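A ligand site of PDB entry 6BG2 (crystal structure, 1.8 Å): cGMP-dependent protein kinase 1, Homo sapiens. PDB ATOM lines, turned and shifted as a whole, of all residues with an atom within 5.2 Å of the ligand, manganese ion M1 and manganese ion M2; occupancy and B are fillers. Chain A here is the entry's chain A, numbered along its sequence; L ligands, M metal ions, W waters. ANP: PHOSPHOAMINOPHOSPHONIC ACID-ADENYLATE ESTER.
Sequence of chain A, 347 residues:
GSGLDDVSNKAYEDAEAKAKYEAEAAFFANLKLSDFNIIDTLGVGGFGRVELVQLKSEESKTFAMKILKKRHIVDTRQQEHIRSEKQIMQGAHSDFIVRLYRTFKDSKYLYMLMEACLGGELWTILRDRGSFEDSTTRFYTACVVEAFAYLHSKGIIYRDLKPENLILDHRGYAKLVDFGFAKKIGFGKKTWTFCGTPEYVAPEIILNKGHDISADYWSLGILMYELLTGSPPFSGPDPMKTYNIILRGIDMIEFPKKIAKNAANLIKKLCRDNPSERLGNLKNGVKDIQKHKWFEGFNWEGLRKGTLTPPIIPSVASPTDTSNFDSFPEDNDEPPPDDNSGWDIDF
The side-chain amino group (NZ) of Lys 66 lies within salt-bridge range of an oxygen (O2A) of the ligand (3.3 Å). The backbone NH of Cys 117 is in hydrogen-bond range of a nitrogen (N1) of the ligand (3.2 Å). The backbone carbonyl oxygen (O) of Glu 115 sits at hydrogen-bond distance from a nitrogen (N6) of the ligand, 2.8 Å away. O2' of the ligand is in hydrogen-bond range of OE2 of Glu 121 (2.6 Å).
The backbone carbonyl oxygen (O) of Asn 165 is in hydrogen-bond range of the backbone NH (N) of Val 177, 3.0 Å away. N of Val 50 sits at hydrogen-bond distance from O of Gly 43 (2.8 Å). The backbone carbonyl oxygen (O) of Ala 64 sits at hydrogen-bond distance from the backbone NH (N) of Met 114, at 2.8 Å. O of Val 50 lies within hydrogen-bond range of N of Leu 42 (2.7 Å). The side-chain amide oxygen of Asn 165 lies close to the side-chain carboxylate of Asp 178 (3.3 Å). The side-chain amide nitrogen (ND2) of Asn 165 is in hydrogen-bond range of the backbone carbonyl oxygen (O) of Asp 160, at 2.7 Å. The side-chain amino group (NZ) of Lys 66 lies within salt-bridge range of the side-chain carboxylate (OE1) of Glu 85, at 2.9 Å.
Merely in contact with the ligand: Phe 47 (3.1 Å), Val 50 (3.4 Å), Ala 64 (3.4 Å), Val 98 (3.5 Å), Phe 325 (3.5 Å), Met 114 (3.6 Å), Val 177 (3.7 Å), Leu 42 (3.9 Å) and Ala 116 (3.9 Å). Along chain A the residues within 4 Å of the ligand span positions 42 to 325. The nearest printed residue that does not touch the ligand is Gly 43 (4.2 Å).
The nearest printed residue that does not touch manganese ion M1 is Asn 165 (4.7 Å).
Along chain A the residues within 4 Å of manganese ion M2 span positions 165 to 178. The nearest printed residue that does not touch manganese ion M2 is Glu 164 (4.5 Å).
Manganese ion M1 is bound by O1B of the ligand (2.2 Å), OD1 of Asp 178 (2.3 Å) and O1G of the ligand (2.6 Å). Manganese ion M1 has three donor atoms within binding distance. Slightly farther from manganese ion M1 lies water W4 (2.7 Å).
OD1 of Asp 178 binds manganese ion M2. Manganese ion M2 is bound by O1A of the ligand (2.7 Å). Slightly farther from manganese ion M2 lies the side-chain amide oxygen (OD1) of Asn 165 (2.7 Å). Slightly farther from manganese ion M2 lies O1G of the ligand (2.9 Å).
Water W1 bridges an oxygen (O2') of the ligand (2.6 Å) and the backbone carbonyl oxygen (O) of Leu 42 (2.7 Å). Water W3 lies within hydrogen-bond range of an oxygen (O2B) of the ligand (2.6 Å) and the side-chain amino group (NZ) of Lys 66 (3.0 Å). Water W2 lies within hydrogen-bond range of O2A of the ligand (2.6 Å), NZ of Lys 66 (3.4 Å) and SD of Met 114 (3.5 Å). Water W7 lies within hydrogen-bond range of an oxygen (O3') of the ligand and the backbone carbonyl oxygen of Glu 164. Water W6 lies within hydrogen-bond range of OD1 of Asp 160 and NZ of Lys 162. Water W5 lies within hydrogen-bond range of the side-chain carboxylate (OE2) of Glu 121 (2.5 Å), the backbone carbonyl oxygen (O) of Glu 164 (3.2 Å) and an oxygen (O3') of the ligand (3.4 Å).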
ATOM      1  N   LEU A  42      -5.974   2.714  11.145  1.00  0.00           N
ATOM      2  CA  LEU A  42      -6.600   1.955  12.237  1.00  0.00           C
ATOM      3  C   LEU A  42      -6.666   2.736  13.544  1.00  0.00           C
ATOM      4  O   LEU A  42      -7.601   2.536  14.322  1.00  0.00           O
ATOM      5  CB  LEU A  42      -5.868   0.630  12.452  1.00  0.00           C
ATOM      6  CG  LEU A  42      -5.887  -0.320  11.257  1.00  0.00           C
ATOM      7  CD1 LEU A  42      -4.906  -1.457  11.425  1.00  0.00           C
ATOM      8  CD2 LEU A  42      -7.296  -0.853  10.994  1.00  0.00           C
ATOM      9  N   GLY A  43      -5.685   3.599  13.824  1.00  0.00           N
ATOM     10  CA  GLY A  43      -5.686   4.393  15.031  1.00  0.00           C
ATOM     11  C   GLY A  43      -4.728   5.553  14.884  1.00  0.00           C
ATOM     12  O   GLY A  43      -3.805   5.518  14.074  1.00  0.00           O
ATOM     13  N   VAL A  44      -4.982   6.603  15.671  1.00  0.00           N
ATOM     14  CA  VAL A  44      -4.156   7.808  15.684  1.00  0.00           C
ATOM     15  C   VAL A  44      -3.893   8.229  17.123  1.00  0.00           C
ATOM     16  O   VAL A  44      -4.371   7.600  18.080  1.00  0.00           O
ATOM     17  CB  VAL A  44      -4.802   8.974  14.903  1.00  0.00           C
ATOM     18  CG2 VAL A  44      -5.063   8.573  13.456  1.00  0.00           C
ATOM     19  N   PHE A  47       1.219   9.747  19.711  1.00  0.00           N
ATOM     20  CA  PHE A  47       2.306   8.797  19.507  1.00  0.00           C
ATOM     21  C   PHE A  47       2.595   8.556  18.046  1.00  0.00           C
ATOM     22  O   PHE A  47       3.721   8.195  17.682  1.00  0.00           O
ATOM     23  CB  PHE A  47       1.915   7.447  20.131  1.00  0.00           C
ATOM     24  CG  PHE A  47       0.772   6.765  19.414  1.00  0.00           C
ATOM     25  CD1 PHE A  47       1.001   5.805  18.443  1.00  0.00           C
ATOM     26  CD2 PHE A  47      -0.546   7.124  19.695  1.00  0.00           C
ATOM     27  CE1 PHE A  47      -0.053   5.189  17.778  1.00  0.00           C
ATOM     28  CE2 PHE A  47      -1.601   6.508  19.030  1.00  0.00           C
ATOM     29  CZ  PHE A  47      -1.354   5.540  18.071  1.00  0.00           C
ATOM     30  N   VAL A  50      -1.428   4.176  13.436  1.00  0.00           N
ATOM     31  CA  VAL A  50      -1.412   2.772  13.045  1.00  0.00           C
ATOM     32  C   VAL A  50      -2.185   2.704  11.741  1.00  0.00           C
ATOM     33  O   VAL A  50      -3.385   3.018  11.701  1.00  0.00           O
ATOM     34  CB  VAL A  50      -2.027   1.853  14.108  1.00  0.00           C
ATOM     35  CG1 VAL A  50      -1.982   0.405  13.658  1.00  0.00           C
ATOM     36  CG2 VAL A  50      -1.314   2.032  15.434  1.00  0.00           C
ATOM     37  N   ALA A  64      -0.795  -4.336  10.048  1.00  0.00           N
ATOM     38  CA  ALA A  64      -0.934  -3.103  10.812  1.00  0.00           C
ATOM     39  C   ALA A  64       0.463  -2.519  10.998  1.00  0.00           C
ATOM     40  O   ALA A  64       1.310  -3.129  11.650  1.00  0.00           O
ATOM     41  CB  ALA A  64      -1.591  -3.343  12.161  1.00  0.00           C
ATOM     42  N   LYS A  66       2.487   0.298  12.669  1.00  0.00           N
ATOM     43  CA  LYS A  66       2.520   1.376  13.641  1.00  0.00           C
ATOM     44  C   LYS A  66       3.665   2.308  13.272  1.00  0.00           C
ATOM     45  O   LYS A  66       4.817   1.876  13.170  1.00  0.00           O
ATOM     46  CB  LYS A  66       2.664   0.851  15.074  1.00  0.00           C
ATOM     47  CG  LYS A  66       2.565   1.976  16.104  1.00  0.00           C
ATOM     48  CD  LYS A  66       2.285   1.517  17.541  1.00  0.00           C
ATOM     49  CE  LYS A  66       3.008   0.259  17.950  1.00  0.00           C
ATOM     50  NZ  LYS A  66       2.945   0.082  19.442  1.00  0.00           N
ATOM     51  N   LEU A  68       5.609   5.678  14.372  1.00  0.00           N
ATOM     52  CA  LEU A  68       5.805   6.457  15.574  1.00  0.00           C
ATOM     53  C   LEU A  68       6.730   7.623  15.289  1.00  0.00           C
ATOM     54  O   LEU A  68       7.772   7.454  14.650  1.00  0.00           O
ATOM     55  CB  LEU A  68       6.396   5.621  16.716  1.00  0.00           C
ATOM     56  CG  LEU A  68       5.678   4.357  17.182  1.00  0.00           C
ATOM     57  CD1 LEU A  68       6.426   3.762  18.367  1.00  0.00           C
ATOM     58  CD2 LEU A  68       4.263   4.706  17.590  1.00  0.00           C
ATOM     59  N   GLU A  85       9.837  -3.304  23.422  1.00  0.00           N
ATOM     60  CA  GLU A  85       8.666  -3.716  22.649  1.00  0.00           C
ATOM     61  C   GLU A  85       9.095  -4.401  21.366  1.00  0.00           C
ATOM     62  O   GLU A  85       8.575  -5.465  21.013  1.00  0.00           O
ATOM     63  CB  GLU A  85       7.768  -2.521  22.363  1.00  0.00           C
ATOM     64  CG  GLU A  85       6.572  -2.865  21.493  1.00  0.00           C
ATOM     65  CD  GLU A  85       5.566  -1.733  21.408  1.00  0.00           C
ATOM     66  OE1 GLU A  85       4.500  -1.935  20.784  1.00  0.00           O
ATOM     67  OE2 GLU A  85       5.864  -0.641  21.938  1.00  0.00           O
ATOM     68  N   VAL A  98      -0.047 -10.298  19.281  1.00  0.00           N
ATOM     69  CA  VAL A  98       0.103  -9.722  17.952  1.00  0.00           C
ATOM     70  C   VAL A  98       1.549  -9.882  17.482  1.00  0.00           C
ATOM     71  O   VAL A  98       2.481  -9.461  18.164  1.00  0.00           O
ATOM     72  CB  VAL A  98      -0.311  -8.242  17.951  1.00  0.00           C
ATOM     73  CG1 VAL A  98      -0.138  -7.641  16.555  1.00  0.00           C
ATOM     74  CG2 VAL A  98      -1.759  -8.092  18.393  1.00  0.00           C
ATOM     75  N   MET A 114       3.223  -5.126  11.875  1.00  0.00           N
ATOM     76  CA  MET A 114       2.602  -6.095  12.761  1.00  0.00           C
ATOM     77  C   MET A 114       1.496  -6.831  12.039  1.00  0.00           C
ATOM     78  O   MET A 114       0.987  -6.408  10.997  1.00  0.00           O
ATOM     79  CB  MET A 114       2.010  -5.448  14.016  1.00  0.00           C
ATOM     80  CG  MET A 114       2.936  -4.604  14.846  1.00  0.00           C
ATOM     81  SD  MET A 114       1.961  -3.864  16.177  1.00  0.00           S
ATOM     82  CE  MET A 114       1.306  -2.444  15.302  1.00  0.00           C
ATOM     83  N   GLU A 115       1.128  -7.963  12.638  1.00  0.00           N
ATOM     84  CA  GLU A 115      -0.071  -8.680  12.227  1.00  0.00           C
ATOM     85  C   GLU A 115      -1.283  -7.772  12.419  1.00  0.00           C
ATOM     86  O   GLU A 115      -1.416  -7.101  13.443  1.00  0.00           O
ATOM     87  CB  GLU A 115      -0.196  -9.955  13.052  1.00  0.00           C
ATOM     88  CG  GLU A 115      -1.582 -10.530  13.178  1.00  0.00           C
ATOM     89  CD  GLU A 115      -1.645 -11.615  14.242  1.00  0.00           C
ATOM     90  OE1 GLU A 115      -0.709 -11.713  15.063  1.00  0.00           O
ATOM     91  OE2 GLU A 115      -2.631 -12.381  14.225  1.00  0.00           O
ATOM     92  N   ALA A 116      -2.159  -7.731  11.419  1.00  0.00           N
ATOM     93  CA  ALA A 116      -3.371  -6.934  11.519  1.00  0.00           C
ATOM     94  C   ALA A 116      -4.458  -7.760  12.200  1.00  0.00           C
ATOM     95  O   ALA A 116      -4.733  -8.890  11.795  1.00  0.00           O
ATOM     96  CB  ALA A 116      -3.856  -6.482  10.145  1.00  0.00           C
ATOM     97  N   CYS A 117      -5.084  -7.176  13.217  1.00  0.00           N
ATOM     98  CA  CYS A 117      -6.212  -7.816  13.895  1.00  0.00           C
ATOM     99  C   CYS A 117      -7.425  -6.962  13.560  1.00  0.00           C
ATOM    100  O   CYS A 117      -7.653  -5.914  14.166  1.00  0.00           O
ATOM    101  CB  CYS A 117      -5.958  -7.895  15.403  1.00  0.00           C
ATOM    102  SG  CYS A 117      -4.578  -8.985  15.804  1.00  0.00           S
ATOM    103  N   GLU A 121     -11.246  -3.396  18.623  1.00  0.00           N
ATOM    104  CA  GLU A 121     -10.861  -3.278  20.020  1.00  0.00           C
ATOM    105  C   GLU A 121     -11.898  -3.885  20.950  1.00  0.00           C
ATOM    106  O   GLU A 121     -13.111  -3.733  20.748  1.00  0.00           O
ATOM    107  CB  GLU A 121     -10.683  -1.798  20.392  1.00  0.00           C
ATOM    108  CG  GLU A 121      -9.954  -0.951  19.379  1.00  0.00           C
ATOM    109  CD  GLU A 121      -9.667   0.444  19.909  1.00  0.00           C
ATOM    110  OE1 GLU A 121     -10.638   1.222  20.099  1.00  0.00           O
ATOM    111  OE2 GLU A 121      -8.485   0.743  20.168  1.00  0.00           O
ATOM    112  N   ASP A 160       0.981  -4.660  31.368  1.00  0.00           N
ATOM    113  CA  ASP A 160      -0.004  -3.652  30.988  1.00  0.00           C
ATOM    114  C   ASP A 160      -1.327  -4.300  30.607  1.00  0.00           C
ATOM    115  O   ASP A 160      -2.014  -3.860  29.672  1.00  0.00           O
ATOM    116  CB  ASP A 160       0.514  -2.779  29.845  1.00  0.00           C
ATOM    117  CG  ASP A 160      -0.172  -1.428  29.794  1.00  0.00           C
ATOM    118  OD1 ASP A 160      -0.082  -0.756  28.751  1.00  0.00           O
ATOM    119  OD2 ASP A 160      -0.799  -1.038  30.806  1.00  0.00           O
ATOM    120  N   LYS A 162      -5.085  -4.861  30.518  1.00  0.00           N
ATOM    121  CA  LYS A 162      -6.308  -4.077  30.669  1.00  0.00           C
ATOM    122  C   LYS A 162      -7.101  -4.301  29.390  1.00  0.00           C
ATOM    123  O   LYS A 162      -6.509  -4.698  28.375  1.00  0.00           O
ATOM    124  CB  LYS A 162      -6.005  -2.594  30.897  1.00  0.00           C
ATOM    125  CG  LYS A 162      -5.135  -1.974  29.817  1.00  0.00           C
ATOM    126  CD  LYS A 162      -4.885  -0.511  30.102  1.00  0.00           C
ATOM    127  CE  LYS A 162      -3.866   0.053  29.139  1.00  0.00           C
ATOM    128  NZ  LYS A 162      -3.709   1.521  29.329  1.00  0.00           N
ATOM    129  N   GLU A 164      -8.112  -2.447  27.160  1.00  0.00           N
ATOM    130  CA  GLU A 164      -7.622  -1.631  26.050  1.00  0.00           C
ATOM    131  C   GLU A 164      -6.469  -2.286  25.307  1.00  0.00           C
ATOM    132  O   GLU A 164      -6.252  -1.975  24.129  1.00  0.00           O
ATOM    133  CB  GLU A 164      -7.180  -0.269  26.552  1.00  0.00           C
ATOM    134  CG  GLU A 164      -8.276   0.553  27.072  1.00  0.00           C
ATOM    135  CD  GLU A 164      -8.537   0.382  28.555  1.00  0.00           C
ATOM    136  OE1 GLU A 164      -8.460  -0.770  29.045  1.00  0.00           O
ATOM    137  OE2 GLU A 164      -8.807   1.400  29.237  1.00  0.00           O
ATOM    138  N   ASN A 165      -5.761  -3.216  25.943  1.00  0.00           N
ATOM    139  CA  ASN A 165      -4.639  -3.868  25.305  1.00  0.00           C
ATOM    140  C   ASN A 165      -4.982  -5.242  24.761  1.00  0.00           C
ATOM    141  O   ASN A 165      -4.094  -6.023  24.431  1.00  0.00           O
ATOM    142  CB  ASN A 165      -3.459  -3.925  26.280  1.00  0.00           C
ATOM    143  CG  ASN A 165      -2.752  -2.591  26.385  1.00  0.00           C
ATOM    144  OD1 ASN A 165      -3.014  -1.671  25.606  1.00  0.00           O
ATOM    145  ND2 ASN A 165      -1.852  -2.465  27.352  1.00  0.00           N
ATOM    146  N   ILE A 167      -7.018  -6.982  21.614  1.00  0.00           N
ATOM    147  CA  ILE A 167      -7.590  -6.688  20.302  1.00  0.00           C
ATOM    148  C   ILE A 167      -8.035  -7.998  19.678  1.00  0.00           C
ATOM    149  O   ILE A 167      -7.437  -9.053  19.909  1.00  0.00           O
ATOM    150  CB  ILE A 167      -6.576  -5.934  19.403  1.00  0.00           C
ATOM    151  CG1 ILE A 167      -7.278  -5.350  18.163  1.00  0.00           C
ATOM    152  CG2 ILE A 167      -5.405  -6.825  19.031  1.00  0.00           C
ATOM    153  N   VAL A 177      -1.792  -6.730  22.593  1.00  0.00           N
ATOM    154  CA  VAL A 177      -1.098  -5.690  21.861  1.00  0.00           C
ATOM    155  C   VAL A 177      -0.486  -4.732  22.887  1.00  0.00           C
ATOM    156  O   VAL A 177      -0.799  -4.796  24.069  1.00  0.00           O
ATOM    157  CB  VAL A 177      -2.053  -4.952  20.895  1.00  0.00           C
ATOM    158  CG1 VAL A 177      -2.975  -4.001  21.655  1.00  0.00           C
ATOM    159  CG2 VAL A 177      -1.291  -4.249  19.772  1.00  0.00           C
ATOM    160  N   ASP A 178       0.377  -3.838  22.413  1.00  0.00           N
ATOM    161  CA  ASP A 178       0.994  -2.805  23.252  1.00  0.00           C
ATOM    162  C   ASP A 178       1.914  -3.408  24.301  1.00  0.00           C
ATOM    163  O   ASP A 178       1.501  -3.723  25.419  1.00  0.00           O
ATOM    164  CB  ASP A 178      -0.063  -1.928  23.923  1.00  0.00           C
ATOM    165  CG  ASP A 178       0.552  -0.711  24.612  1.00  0.00           C
ATOM    166  OD1 ASP A 178      -0.215   0.109  25.153  1.00  0.00           O
ATOM    167  OD2 ASP A 178       1.787  -0.550  24.587  1.00  0.00           O
ATOM    168  N   PHE A 325     -13.096  -0.492  12.971  1.00  0.00           N
ATOM    169  CA  PHE A 325     -12.304   0.566  13.567  1.00  0.00           C
ATOM    170  C   PHE A 325     -12.923   1.923  13.265  1.00  0.00           C
ATOM    171  O   PHE A 325     -13.664   2.079  12.297  1.00  0.00           O
ATOM    172  CB  PHE A 325     -10.850   0.509  13.081  1.00  0.00           C
ATOM    173  CG  PHE A 325     -10.111  -0.717  13.544  1.00  0.00           C
ATOM    174  CD1 PHE A 325     -10.235  -1.918  12.863  1.00  0.00           C
ATOM    175  CD2 PHE A 325      -9.305  -0.671  14.680  1.00  0.00           C
ATOM    176  CE1 PHE A 325      -9.561  -3.053  13.291  1.00  0.00           C
ATOM    177  CE2 PHE A 325      -8.630  -1.806  15.108  1.00  0.00           C
ATOM    178  CZ  PHE A 325      -8.766  -2.989  14.422  1.00  0.00           C
HETATM  179  PG  ANP L   1      -1.916   4.658  22.657  1.00  0.00           P
HETATM  180  O1G ANP L   1      -2.571   3.362  23.278  1.00  0.00           O
HETATM  181  O2G ANP L   1      -0.909   5.220  23.606  1.00  0.00           O
HETATM  182  O3G ANP L   1      -3.051   5.738  22.402  1.00  0.00           O
HETATM  183  PB  ANP L   1       0.105   3.222  21.317  1.00  0.00           P
HETATM  184  O1B ANP L   1       0.210   2.681  22.705  1.00  0.00           O
HETATM  185  O2B ANP L   1       1.434   3.954  20.969  1.00  0.00           O
HETATM  186  N3B ANP L   1      -1.191   4.272  21.176  1.00  0.00           N
HETATM  187  PA  ANP L   1      -1.017   0.816  20.646  1.00  0.00           P
HETATM  188  O1A ANP L   1      -1.709   0.977  21.953  1.00  0.00           O
HETATM  189  O2A ANP L   1      -0.115  -0.413  20.575  1.00  0.00           O
HETATM  190  O3A ANP L   1      -0.092   2.055  20.296  1.00  0.00           O
HETATM  191  O5' ANP L   1      -2.131   0.786  19.506  1.00  0.00           O
HETATM  192  C5' ANP L   1      -2.848   1.965  19.090  1.00  0.00           C
HETATM  193  C4' ANP L   1      -4.206   1.546  18.591  1.00  0.00           C
HETATM  194  O4' ANP L   1      -4.111   1.178  17.191  1.00  0.00           O
HETATM  195  C3' ANP L   1      -4.807   0.330  19.291  1.00  0.00           C
HETATM  196  O3' ANP L   1      -5.572   0.693  20.435  1.00  0.00           O
HETATM  197  C2' ANP L   1      -5.672  -0.286  18.188  1.00  0.00           C
HETATM  198  O2' ANP L   1      -6.968   0.316  18.093  1.00  0.00           O
HETATM  199  C1' ANP L   1      -4.833  -0.015  16.944  1.00  0.00           C
HETATM  200  N9  ANP L   1      -3.878  -1.079  16.672  1.00  0.00           N
HETATM  201  C8  ANP L   1      -2.597  -1.212  17.143  1.00  0.00           C
HETATM  202  N7  ANP L   1      -1.983  -2.295  16.737  1.00  0.00           N
HETATM  203  C5  ANP L   1      -2.926  -2.929  15.951  1.00  0.00           C
HETATM  204  C6  ANP L   1      -2.901  -4.143  15.230  1.00  0.00           C
HETATM  205  N6  ANP L   1      -1.846  -4.959  15.186  1.00  0.00           N
HETATM  206  N1  ANP L   1      -4.015  -4.485  14.549  1.00  0.00           N
HETATM  207  C2  ANP L   1      -5.076  -3.680  14.587  1.00  0.00           C
HETATM  208  N3  ANP L   1      -5.217  -2.517  15.238  1.00  0.00           N
HETATM  209  C4  ANP L   1      -4.100  -2.204  15.904  1.00  0.00           C
HETATM  210 MN    MN M   1      -0.666   2.301  24.688  1.00  0.00          MN
HETATM  211 MN    MN M   2      -2.677   0.745  24.432  1.00  0.00          MN
HETATM  212  O   HOH W   1      -8.049   2.375  16.940  1.00  0.00           O
HETATM  213  O   HOH W   2       0.310  -1.776  18.377  1.00  0.00           O
HETATM  214  O   HOH W   3       3.578   2.468  21.068  1.00  0.00           O
HETATM  215  O   HOH W   4       1.962   1.895  24.218  1.00  0.00           O
HETATM  216  O   HOH W   5      -8.101  -1.263  21.659  1.00  0.00           O
HETATM  217  O   HOH W   6      -0.619   1.449  27.755  1.00  0.00           O
HETATM  218  O   HOH W   7      -3.931  -0.870  22.289  1.00  0.00           O
HETATM  219  O   HOH W   8      -5.540   5.567  23.687  1.00  0.00           O
